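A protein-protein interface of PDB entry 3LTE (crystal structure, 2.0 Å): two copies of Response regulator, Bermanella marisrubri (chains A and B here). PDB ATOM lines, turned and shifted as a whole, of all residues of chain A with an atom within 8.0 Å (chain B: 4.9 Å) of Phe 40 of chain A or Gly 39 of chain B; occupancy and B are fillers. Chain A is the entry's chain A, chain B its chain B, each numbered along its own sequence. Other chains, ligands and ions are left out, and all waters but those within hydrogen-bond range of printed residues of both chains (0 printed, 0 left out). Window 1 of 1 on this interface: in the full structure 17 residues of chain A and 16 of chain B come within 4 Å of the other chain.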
ATOM      1  N   VAL A  12     -23.995 -12.793  20.530  1.00  0.00           N
ATOM      2  CA  VAL A  12     -22.996 -11.957  19.862  1.00  0.00           C
ATOM      3  C   VAL A  12     -23.513 -11.508  18.498  1.00  0.00           C
ATOM      4  O   VAL A  12     -23.657 -12.317  17.569  1.00  0.00           O
ATOM      5  CB  VAL A  12     -21.621 -12.661  19.715  1.00  0.00           C
ATOM      6  CG1 VAL A  12     -20.600 -11.719  19.085  1.00  0.00           C
ATOM      7  CG2 VAL A  12     -21.117 -13.147  21.059  1.00  0.00           C
ATOM      8  N   ALA A  36     -23.046  -8.940  23.406  1.00  0.00           N
ATOM      9  CA  ALA A  36     -21.805  -8.305  22.992  1.00  0.00           C
ATOM     10  C   ALA A  36     -21.941  -7.898  21.536  1.00  0.00           C
ATOM     11  O   ALA A  36     -22.315  -8.716  20.704  1.00  0.00           O
ATOM     12  CB  ALA A  36     -20.660  -9.273  23.154  1.00  0.00           C
ATOM     13  N   HIS A  37     -21.639  -6.639  21.231  1.00  0.00           N
ATOM     14  CA  HIS A  37     -21.681  -6.145  19.851  1.00  0.00           C
ATOM     15  C   HIS A  37     -20.329  -6.246  19.156  1.00  0.00           C
ATOM     16  O   HIS A  37     -20.203  -5.926  17.968  1.00  0.00           O
ATOM     17  CB  HIS A  37     -22.213  -4.709  19.799  1.00  0.00           C
ATOM     18  CG  HIS A  37     -23.495  -4.516  20.550  1.00  0.00           C
ATOM     19  ND1 HIS A  37     -24.695  -5.041  20.118  1.00  0.00           N
ATOM     20  CD2 HIS A  37     -23.760  -3.871  21.709  1.00  0.00           C
ATOM     21  CE1 HIS A  37     -25.646  -4.722  20.979  1.00  0.00           C
ATOM     22  NE2 HIS A  37     -25.105  -4.013  21.954  1.00  0.00           N
ATOM     23  N   ASN A  38     -19.321  -6.701  19.896  1.00  0.00           N
ATOM     24  CA  ASN A  38     -17.971  -6.803  19.357  1.00  0.00           C
ATOM     25  C   ASN A  38     -17.194  -8.015  19.902  1.00  0.00           C
ATOM     26  O   ASN A  38     -17.593  -8.624  20.898  1.00  0.00           O
ATOM     27  CB  ASN A  38     -17.206  -5.481  19.590  1.00  0.00           C
ATOM     28  CG  ASN A  38     -17.074  -5.130  21.078  1.00  0.00           C
ATOM     29  OD1 ASN A  38     -16.310  -5.757  21.802  1.00  0.00           O
ATOM     30  ND2 ASN A  38     -17.808  -4.117  21.524  1.00  0.00           N
ATOM     31  N   GLY A  39     -16.086  -8.342  19.239  1.00  0.00           N
ATOM     32  CA  GLY A  39     -15.258  -9.496  19.580  1.00  0.00           C
ATOM     33  C   GLY A  39     -14.651  -9.425  20.967  1.00  0.00           C
ATOM     34  O   GLY A  39     -14.684 -10.415  21.715  1.00  0.00           O
ATOM     35  N   PHE A  40     -14.108  -8.256  21.318  1.00  0.00           N
ATOM     36  CA  PHE A  40     -13.493  -8.069  22.628  1.00  0.00           C
ATOM     37  C   PHE A  40     -14.473  -8.341  23.750  1.00  0.00           C
ATOM     38  O   PHE A  40     -14.160  -9.079  24.676  1.00  0.00           O
ATOM     39  CB  PHE A  40     -12.854  -6.680  22.788  1.00  0.00           C
ATOM     40  CG  PHE A  40     -12.152  -6.498  24.102  1.00  0.00           C
ATOM     41  CD1 PHE A  40     -12.771  -5.818  25.151  1.00  0.00           C
ATOM     42  CD2 PHE A  40     -10.873  -7.027  24.300  1.00  0.00           C
ATOM     43  CE1 PHE A  40     -12.127  -5.664  26.371  1.00  0.00           C
ATOM     44  CE2 PHE A  40     -10.215  -6.871  25.506  1.00  0.00           C
ATOM     45  CZ  PHE A  40     -10.845  -6.203  26.555  1.00  0.00           C
ATOM     46  N   ASP A  41     -15.659  -7.746  23.639  1.00  0.00           N
ATOM     47  CA  ASP A  41     -16.712  -7.899  24.635  1.00  0.00           C
ATOM     48  C   ASP A  41     -17.175  -9.354  24.728  1.00  0.00           C
ATOM     49  O   ASP A  41     -17.395  -9.862  25.826  1.00  0.00           O
ATOM     50  CB  ASP A  41     -17.883  -6.964  24.319  1.00  0.00           C
ATOM     51  CG  ASP A  41     -18.612  -6.494  25.567  1.00  0.00           C
ATOM     52  OD1 ASP A  41     -19.726  -5.953  25.423  1.00  0.00           O
ATOM     53  OD2 ASP A  41     -18.081  -6.659  26.689  1.00  0.00           O
ATOM     54  N   ALA A  42     -17.284 -10.014  23.574  1.00  0.00           N
ATOM     55  CA  ALA A  42     -17.565 -11.454  23.491  1.00  0.00           C
ATOM     56  C   ALA A  42     -16.470 -12.278  24.157  1.00  0.00           C
ATOM     57  O   ALA A  42     -16.765 -13.222  24.893  1.00  0.00           O
ATOM     58  CB  ALA A  42     -17.734 -11.884  22.039  1.00  0.00           C
ATOM     59  N   GLY A  43     -15.216 -11.910  23.894  1.00  0.00           N
ATOM     60  CA  GLY A  43     -14.059 -12.521  24.536  1.00  0.00           C
ATOM     61  C   GLY A  43     -14.084 -12.418  26.050  1.00  0.00           C
ATOM     62  O   GLY A  43     -13.806 -13.392  26.747  1.00  0.00           O
ATOM     63  N   ILE A  44     -14.439 -11.241  26.561  1.00  0.00           N
ATOM     64  CA  ILE A  44     -14.455 -11.017  28.003  1.00  0.00           C
ATOM     65  C   ILE A  44     -15.607 -11.763  28.672  1.00  0.00           C
ATOM     66  O   ILE A  44     -15.396 -12.507  29.637  1.00  0.00           O
ATOM     67  CB  ILE A  44     -14.496  -9.505  28.344  1.00  0.00           C
ATOM     68  CG1 ILE A  44     -13.181  -8.820  27.928  1.00  0.00           C
ATOM     69  CG2 ILE A  44     -14.785  -9.281  29.831  1.00  0.00           C
ATOM     70  CD1 ILE A  44     -11.943  -9.249  28.701  1.00  0.00           C
ATOM     71  N   LYS A  45     -16.812 -11.596  28.122  1.00  0.00           N
ATOM     72  CA  LYS A  45     -18.026 -12.211  28.663  1.00  0.00           C
ATOM     73  C   LYS A  45     -18.022 -13.737  28.670  1.00  0.00           C
ATOM     74  O   LYS A  45     -18.767 -14.360  29.423  1.00  0.00           O
ATOM     75  CB  LYS A  45     -19.265 -11.659  27.955  1.00  0.00           C
ATOM     76  CG  LYS A  45     -19.604 -10.259  28.407  1.00  0.00           C
ATOM     77  CD  LYS A  45     -20.567  -9.566  27.475  1.00  0.00           C
ATOM     78  CE  LYS A  45     -21.186  -8.379  28.186  1.00  0.00           C
ATOM     79  NZ  LYS A  45     -21.512  -7.250  27.286  1.00  0.00           N
ATOM     80  N   LEU A  46     -17.143 -14.332  27.868  1.00  0.00           N
ATOM     81  CA  LEU A  46     -16.985 -15.782  27.814  1.00  0.00           C
ATOM     82  C   LEU A  46     -16.476 -16.366  29.129  1.00  0.00           C
ATOM     83  O   LEU A  46     -16.793 -17.506  29.469  1.00  0.00           O
ATOM     84  CB  LEU A  46     -16.061 -16.174  26.656  1.00  0.00           C
ATOM     85  CG  LEU A  46     -16.359 -17.475  25.905  1.00  0.00           C
ATOM     86  CD1 LEU A  46     -17.843 -17.667  25.713  1.00  0.00           C
ATOM     87  CD2 LEU A  46     -15.698 -17.430  24.555  1.00  0.00           C
ATOM     88  N   LYS A  62     -17.222  -6.464  11.313  1.00  0.00           N
ATOM     89  CA  LYS A  62     -16.024  -6.254  12.117  1.00  0.00           C
ATOM     90  C   LYS A  62     -15.683  -7.455  13.007  1.00  0.00           C
ATOM     91  O   LYS A  62     -14.774  -7.385  13.835  1.00  0.00           O
ATOM     92  CB  LYS A  62     -16.153  -4.957  12.926  1.00  0.00           C
ATOM     93  CG  LYS A  62     -16.449  -3.761  12.037  1.00  0.00           C
ATOM     94  CD  LYS A  62     -16.081  -2.439  12.652  1.00  0.00           C
ATOM     95  CE  LYS A  62     -15.855  -1.423  11.532  1.00  0.00           C
ATOM     96  NZ  LYS A  62     -15.425  -0.094  12.036  1.00  0.00           N
ATOM     97  N   LEU A  63     -16.418  -8.551  12.820  1.00  0.00           N
ATOM     98  CA  LEU A  63     -16.115  -9.824  13.471  1.00  0.00           C
ATOM     99  C   LEU A  63     -16.228 -11.007  12.501  1.00  0.00           C
ATOM    100  O   LEU A  63     -17.266 -11.226  11.883  1.00  0.00           O
ATOM    101  CB  LEU A  63     -17.013 -10.047  14.699  1.00  0.00           C
ATOM    102  CG  LEU A  63     -16.671 -11.232  15.614  1.00  0.00           C
ATOM    103  CD1 LEU A  63     -15.195 -11.258  15.919  1.00  0.00           C
ATOM    104  CD2 LEU A  63     -17.454 -11.191  16.918  1.00  0.00           C
ATOM    105  N   VAL A  68     -13.153 -16.524  15.525  1.00  0.00           N
ATOM    106  CA  VAL A  68     -13.649 -16.736  16.895  1.00  0.00           C
ATOM    107  C   VAL A  68     -13.591 -18.218  17.261  1.00  0.00           C
ATOM    108  O   VAL A  68     -13.060 -18.579  18.319  1.00  0.00           O
ATOM    109  CB  VAL A  68     -15.083 -16.168  17.113  1.00  0.00           C
ATOM    110  CG1 VAL A  68     -15.722 -16.715  18.391  1.00  0.00           C
ATOM    111  CG2 VAL A  68     -15.036 -14.665  17.177  1.00  0.00           C
ATOM    112  N   HIS B  37      -4.354 -10.253  17.277  1.00  0.00           N
ATOM    113  CA  HIS B  37      -4.537  -9.456  16.048  1.00  0.00           C
ATOM    114  C   HIS B  37      -5.954  -8.909  15.904  1.00  0.00           C
ATOM    115  O   HIS B  37      -6.235  -8.126  15.000  1.00  0.00           O
ATOM    116  CB  HIS B  37      -4.195 -10.272  14.790  1.00  0.00           C
ATOM    117  CG  HIS B  37      -2.771 -10.734  14.717  1.00  0.00           C
ATOM    118  ND1 HIS B  37      -1.699  -9.886  14.894  1.00  0.00           N
ATOM    119  CD2 HIS B  37      -2.244 -11.954  14.454  1.00  0.00           C
ATOM    120  CE1 HIS B  37      -0.575 -10.566  14.757  1.00  0.00           C
ATOM    121  NE2 HIS B  37      -0.878 -11.824  14.494  1.00  0.00           N
ATOM    122  N   ASN B  38      -6.840  -9.344  16.792  1.00  0.00           N
ATOM    123  CA  ASN B  38      -8.252  -8.973  16.777  1.00  0.00           C
ATOM    124  C   ASN B  38      -8.764  -8.880  18.204  1.00  0.00           C
ATOM    125  O   ASN B  38      -8.114  -9.377  19.127  1.00  0.00           O
ATOM    126  CB  ASN B  38      -9.092  -9.994  15.979  1.00  0.00           C
ATOM    127  CG  ASN B  38      -8.989 -11.418  16.528  1.00  0.00           C
ATOM    128  OD1 ASN B  38      -9.580 -11.763  17.562  1.00  0.00           O
ATOM    129  ND2 ASN B  38      -8.253 -12.251  15.822  1.00  0.00           N
ATOM    130  N   GLY B  39      -9.932  -8.264  18.371  1.00  0.00           N
ATOM    131  CA  GLY B  39     -10.535  -8.055  19.689  1.00  0.00           C
ATOM    132  C   GLY B  39     -10.905  -9.309  20.449  1.00  0.00           C
ATOM    133  O   GLY B  39     -10.736  -9.361  21.678  1.00  0.00           O
ATOM    134  N   PHE B  40     -11.418 -10.320  19.742  1.00  0.00           N
ATOM    135  CA  PHE B  40     -11.813 -11.554  20.417  1.00  0.00           C
ATOM    136  C   PHE B  40     -10.624 -12.276  21.034  1.00  0.00           C
ATOM    137  O   PHE B  40     -10.715 -12.750  22.164  1.00  0.00           O
ATOM    138  CB  PHE B  40     -12.619 -12.502  19.520  1.00  0.00           C
ATOM    139  CG  PHE B  40     -13.158 -13.709  20.252  1.00  0.00           C
ATOM    140  CD1 PHE B  40     -12.503 -14.936  20.179  1.00  0.00           C
ATOM    141  CD2 PHE B  40     -14.304 -13.614  21.028  1.00  0.00           C
ATOM    142  CE1 PHE B  40     -12.992 -16.044  20.855  1.00  0.00           C
ATOM    143  CE2 PHE B  40     -14.794 -14.718  21.710  1.00  0.00           C
ATOM    144  CZ  PHE B  40     -14.133 -15.931  21.625  1.00  0.00           C
ATOM    145  N   ASP B  41      -9.519 -12.338  20.297  1.00  0.00           N
ATOM    146  CA  ASP B  41      -8.284 -12.918  20.809  1.00  0.00           C
ATOM    147  C   ASP B  41      -7.732 -12.122  21.979  1.00  0.00           C
ATOM    148  O   ASP B  41      -7.275 -12.710  22.956  1.00  0.00           O
ATOM    149  CB  ASP B  41      -7.230 -13.045  19.710  1.00  0.00           C
ATOM    150  CG  ASP B  41      -6.997 -14.480  19.290  1.00  0.00           C
ATOM    151  OD1 ASP B  41      -6.759 -14.708  18.085  1.00  0.00           O
ATOM    152  OD2 ASP B  41      -7.043 -15.382  20.160  1.00  0.00           O
ATOM    153  N   ALA B  42      -7.813 -10.794  21.885  1.00  0.00           N
ATOM    154  CA  ALA B  42      -7.400  -9.901  22.973  1.00  0.00           C
ATOM    155  C   ALA B  42      -8.161 -10.211  24.255  1.00  0.00           C
ATOM    156  O   ALA B  42      -7.548 -10.392  25.308  1.00  0.00           O
ATOM    157  CB  ALA B  42      -7.591  -8.438  22.574  1.00  0.00           C
ATOM    158  N   GLY B  43      -9.488 -10.295  24.141  1.00  0.00           N
ATOM    159  CA  GLY B  43     -10.362 -10.593  25.276  1.00  0.00           C
ATOM    160  C   GLY B  43     -10.179 -11.979  25.868  1.00  0.00           C
ATOM    161  O   GLY B  43     -10.286 -12.158  27.083  1.00  0.00           O
ATOM    162  N   LEU B  46      -6.647 -12.082  27.654  1.00  0.00           N
ATOM    163  CA  LEU B  46      -6.666 -11.313  28.889  1.00  0.00           C
ATOM    164  C   LEU B  46      -6.972 -12.215  30.094  1.00  0.00           C
ATOM    165  O   LEU B  46      -6.505 -11.944  31.197  1.00  0.00           O
ATOM    166  CB  LEU B  46      -7.667 -10.165  28.778  1.00  0.00           C
ATOM    167  CG  LEU B  46      -7.389  -8.897  29.580  1.00  0.00           C
ATOM    168  CD1 LEU B  46      -7.725  -7.674  28.740  1.00  0.00           C
ATOM    169  CD2 LEU B  46      -8.201  -8.899  30.873  1.00  0.00           C
ATOM    170  N   MET B  54      -1.313  -4.289  28.848  1.00  0.00           N
ATOM    171  CA  MET B  54      -1.829  -4.501  27.500  1.00  0.00           C
ATOM    172  C   MET B  54      -1.532  -3.271  26.641  1.00  0.00           C
ATOM    173  O   MET B  54      -1.883  -2.146  27.011  1.00  0.00           O
ATOM    174  CB  MET B  54      -3.344  -4.805  27.524  1.00  0.00           C
ATOM    175  CG  MET B  54      -3.932  -5.322  26.193  1.00  0.00           C
ATOM    176  SD  MET B  54      -5.755  -5.452  26.122  1.00  0.00           S
ATOM    177  CE  MET B  54      -6.148  -3.720  25.998  1.00  0.00           C
ATOM    178  N   MET B  60      -6.769   0.282  14.681  1.00  0.00           N
ATOM    179  CA  MET B  60      -7.269  -1.005  14.188  1.00  0.00           C
ATOM    180  C   MET B  60      -8.623  -0.768  13.509  1.00  0.00           C
ATOM    181  O   MET B  60      -9.555  -0.304  14.164  1.00  0.00           O
ATOM    182  CB  MET B  60      -7.387  -2.010  15.348  1.00  0.00           C
ATOM    183  CG  MET B  60      -6.052  -2.333  16.046  1.00  0.00           C
ATOM    184  SD  MET B  60      -6.219  -3.322  17.548  1.00  0.00           S
ATOM    185  CE  MET B  60      -6.803  -4.864  16.844  1.00  0.00           C
ATOM    186  N   LEU B  63     -11.366  -2.748  15.302  1.00  0.00           N
ATOM    187  CA  LEU B  63     -11.456  -2.563  16.755  1.00  0.00           C
ATOM    188  C   LEU B  63     -11.447  -1.088  17.177  1.00  0.00           C
ATOM    189  O   LEU B  63     -10.561  -0.324  16.794  1.00  0.00           O
ATOM    190  CB  LEU B  63     -10.341  -3.333  17.481  1.00  0.00           C
ATOM    191  CG  LEU B  63     -10.270  -3.241  19.024  1.00  0.00           C
ATOM    192  CD1 LEU B  63      -9.794  -4.533  19.633  1.00  0.00           C
ATOM    193  CD2 LEU B  63      -9.378  -2.092  19.508  1.00  0.00           C
ATOM    194  N   ASP B  67     -14.096   0.959  22.966  1.00  0.00           N
ATOM    195  CA  ASP B  67     -14.957  -0.169  23.326  1.00  0.00           C
ATOM    196  C   ASP B  67     -14.240  -1.123  24.277  1.00  0.00           C
ATOM    197  O   ASP B  67     -14.859  -1.646  25.192  1.00  0.00           O
ATOM    198  CB  ASP B  67     -15.466  -0.928  22.098  1.00  0.00           C
ATOM    199  CG  ASP B  67     -16.549  -0.177  21.340  1.00  0.00           C
ATOM    200  OD1 ASP B  67     -17.332   0.568  21.968  1.00  0.00           O
ATOM    201  OD2 ASP B  67     -16.626  -0.348  20.106  1.00  0.00           O
ATOM    202  N   VAL B  68     -12.938  -1.326  24.056  1.00  0.00           N
ATOM    203  CA  VAL B  68     -12.105  -2.160  24.930  1.00  0.00           C
ATOM    204  C   VAL B  68     -12.068  -1.593  26.352  1.00  0.00           C
ATOM    205  O   VAL B  68     -12.340  -2.312  27.328  1.00  0.00           O
ATOM    206  CB  VAL B  68     -10.664  -2.312  24.372  1.00  0.00           C
ATOM    207  CG1 VAL B  68      -9.777  -3.080  25.338  1.00  0.00           C
ATOM    208  CG2 VAL B  68     -10.677  -2.997  23.016  1.00  0.00           C
ATOM    209  N   SER B  71     -15.537  -1.730  27.959  1.00  0.00           N
ATOM    210  CA  SER B  71     -15.914  -3.113  28.268  1.00  0.00           C
ATOM    211  C   SER B  71     -15.246  -3.618  29.536  1.00  0.00           C
ATOM    212  O   SER B  71     -15.836  -4.398  30.276  1.00  0.00           O
ATOM    213  CB  SER B  71     -15.575  -4.060  27.123  1.00  0.00           C
ATOM    214  OG  SER B  71     -15.878  -5.395  27.491  1.00  0.00           O
ATOM    215  N   LEU B  72     -14.007  -3.180  29.755  1.00  0.00           N
ATOM    216  CA  LEU B  72     -13.267  -3.483  30.967  1.00  0.00           C
ATOM    217  C   LEU B  72     -13.913  -2.836  32.194  1.00  0.00           C
ATOM    218  O   LEU B  72     -14.000  -3.481  33.236  1.00  0.00           O
ATOM    219  CB  LEU B  72     -11.813  -3.038  30.828  1.00  0.00           C
ATOM    220  CG  LEU B  72     -10.684  -4.032  30.513  1.00  0.00           C
ATOM    221  CD1 LEU B  72     -11.130  -5.431  30.102  1.00  0.00           C
ATOM    222  CD2 LEU B  72      -9.744  -3.436  29.467  1.00  0.00           C
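The side-chain carboxylate of Asp 41 of chain A sits at hydrogen-bond distance from the side-chain hydroxyl of Ser 71 of chain B (2.7 Å).
N of Phe 40 of chain A sits at hydrogen-bond distance from OD1 of Asn 38 of chain A (3.4 Å). OD1 of Asn 38 of chain A sits at hydrogen-bond distance from N of Asp 41 of chain A, at 2.8 Å. The side-chain amino group of Lys 45 of chain A is in salt-bridge range of the side-chain carboxylate of Asp 41 of chain A (2.9 Å). The side-chain amide oxygen of Asn 38 of chain B sits at hydrogen-bond distance from the backbone NH of Phe 40 of chain B.
C of Gly 39 of chain A touches C of Gly 39 of chain B, 3.8 Å away. O of Gly 39 of chain B touches CA of Phe 40 of chain A, 3.2 Å away. N of Phe 40 of chain A touches N of Phe 40 of chain B, at 3.7 Å. Phe 40 of chain A touches Ala 42 of chain B. Gly 43 of chain B touches Phe 40 of chain A (N to CD2, 3.6 Å). Leu 72 of chain B touches Phe 40 of chain A (CD1 to CZ, 3.6 Å). C of Ala 42 of chain A touches CE2 of Phe 40 of chain B, at 3.8 Å. O of Gly 43 of chain B touches O of Gly 43 of chain A, 3.7 Å away. Ile 44 of chain A touches Gly 43 of chain B. Leu 46 of chain A touches Phe 40 of chain B (CD2 to CZ, 3.6 Å).
Of chain B, only Gly 39 (3.2 Å), Phe 40 (3.7 Å), Ala 42 (3.97 Å), Gly 43 (3.6 Å), Val 68 (3.5 Å), Ser 71 (3.9 Å) and Leu 72 (3.6 Å) come within 4 Å of Phe 40 of chain A. Printed residues of chain B within 4 Å of Ala 42 of chain A: Phe 40. Of the printed residues of chain B, Ile 44 of chain A touches Gly 43 (3.7 Å). Asn 38 of chain B touches none of the printed residues of chain A. Gly 39 of chain B touches just these residues of chain A: Gly 39 (3.8 Å) and Phe 40 (3.2 Å). Of the printed residues of chain A, Phe 40 of chain B touches Gly 39 (3.3 Å), Phe 40 (3.7 Å), Ala 42 (3.8 Å), Gly 43 (3.5 Å), Leu 46 (3.6 Å) and Val 68 (3.6 Å). Printed residues of chain A within 4 Å of Ala 42 of chain B: Phe 40. Of the printed residues of chain A, Gly 43 of chain B touches Phe 40, Gly 43 and Ile 44. The nearest residue of chain A that does not touch Gly 39 of chain B is Gly 43 of chain A (5.4 Å). The nearest printed residue of chain A that does not touch Phe 40 of chain B is Leu 63 of chain A (4.6 Å).
Printed residues of chain B that touch a printed residue of chain A: Gly 39, Phe 40, Ala 42, Gly 43, Asp 67, Val 68, Ser 71 and Leu 72. Hydrophobic or aromatic side chains of chain B that line the printed part of chain A: Phe 40, Ala 42, Val 68 and Leu 72. Of the 15 printed residues of chain A, 9 touch a printed residue of chain B. Printed residues of chain A that touch a printed residue of chain B: Asn 38, Gly 39, Phe 40, Asp 41, Ala 42, Gly 43, Ile 44, Leu 46 and Val 68. Hydrophobic or aromatic side chains of chain A within 4 Å of the printed part of chain B: Phe 40, Ala 42, Ile 44, Leu 46 and Val 68. Among the printed residues, no Asp or Glu carboxylate lies within 4 Å of a Lys or Arg side-chain nitrogen of the other chain.
Gly 39 of chain A touches its own counterpart, Gly 39 of chain B. Phe 40 of chain A touches Gly 43 of chain B, and with the chains exchanged Gly 43 of chain A touches Phe 40 of chain B. Phe 40 of chain A touches Val 68 of chain B, and with the chains exchanged Val 68 of chain A touches Phe 40 of chain B. Leu 46 of chain A touches Phe 40 of chain B, but with the chains exchanged Phe 40 of chain A does not touch Leu 46 of chain B (4.1 Å). 10 positions are printed for both chains. Of the 17 pairs that touch across the chains among the printed residues, 11 have their exchanged pair printed and touching as well.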
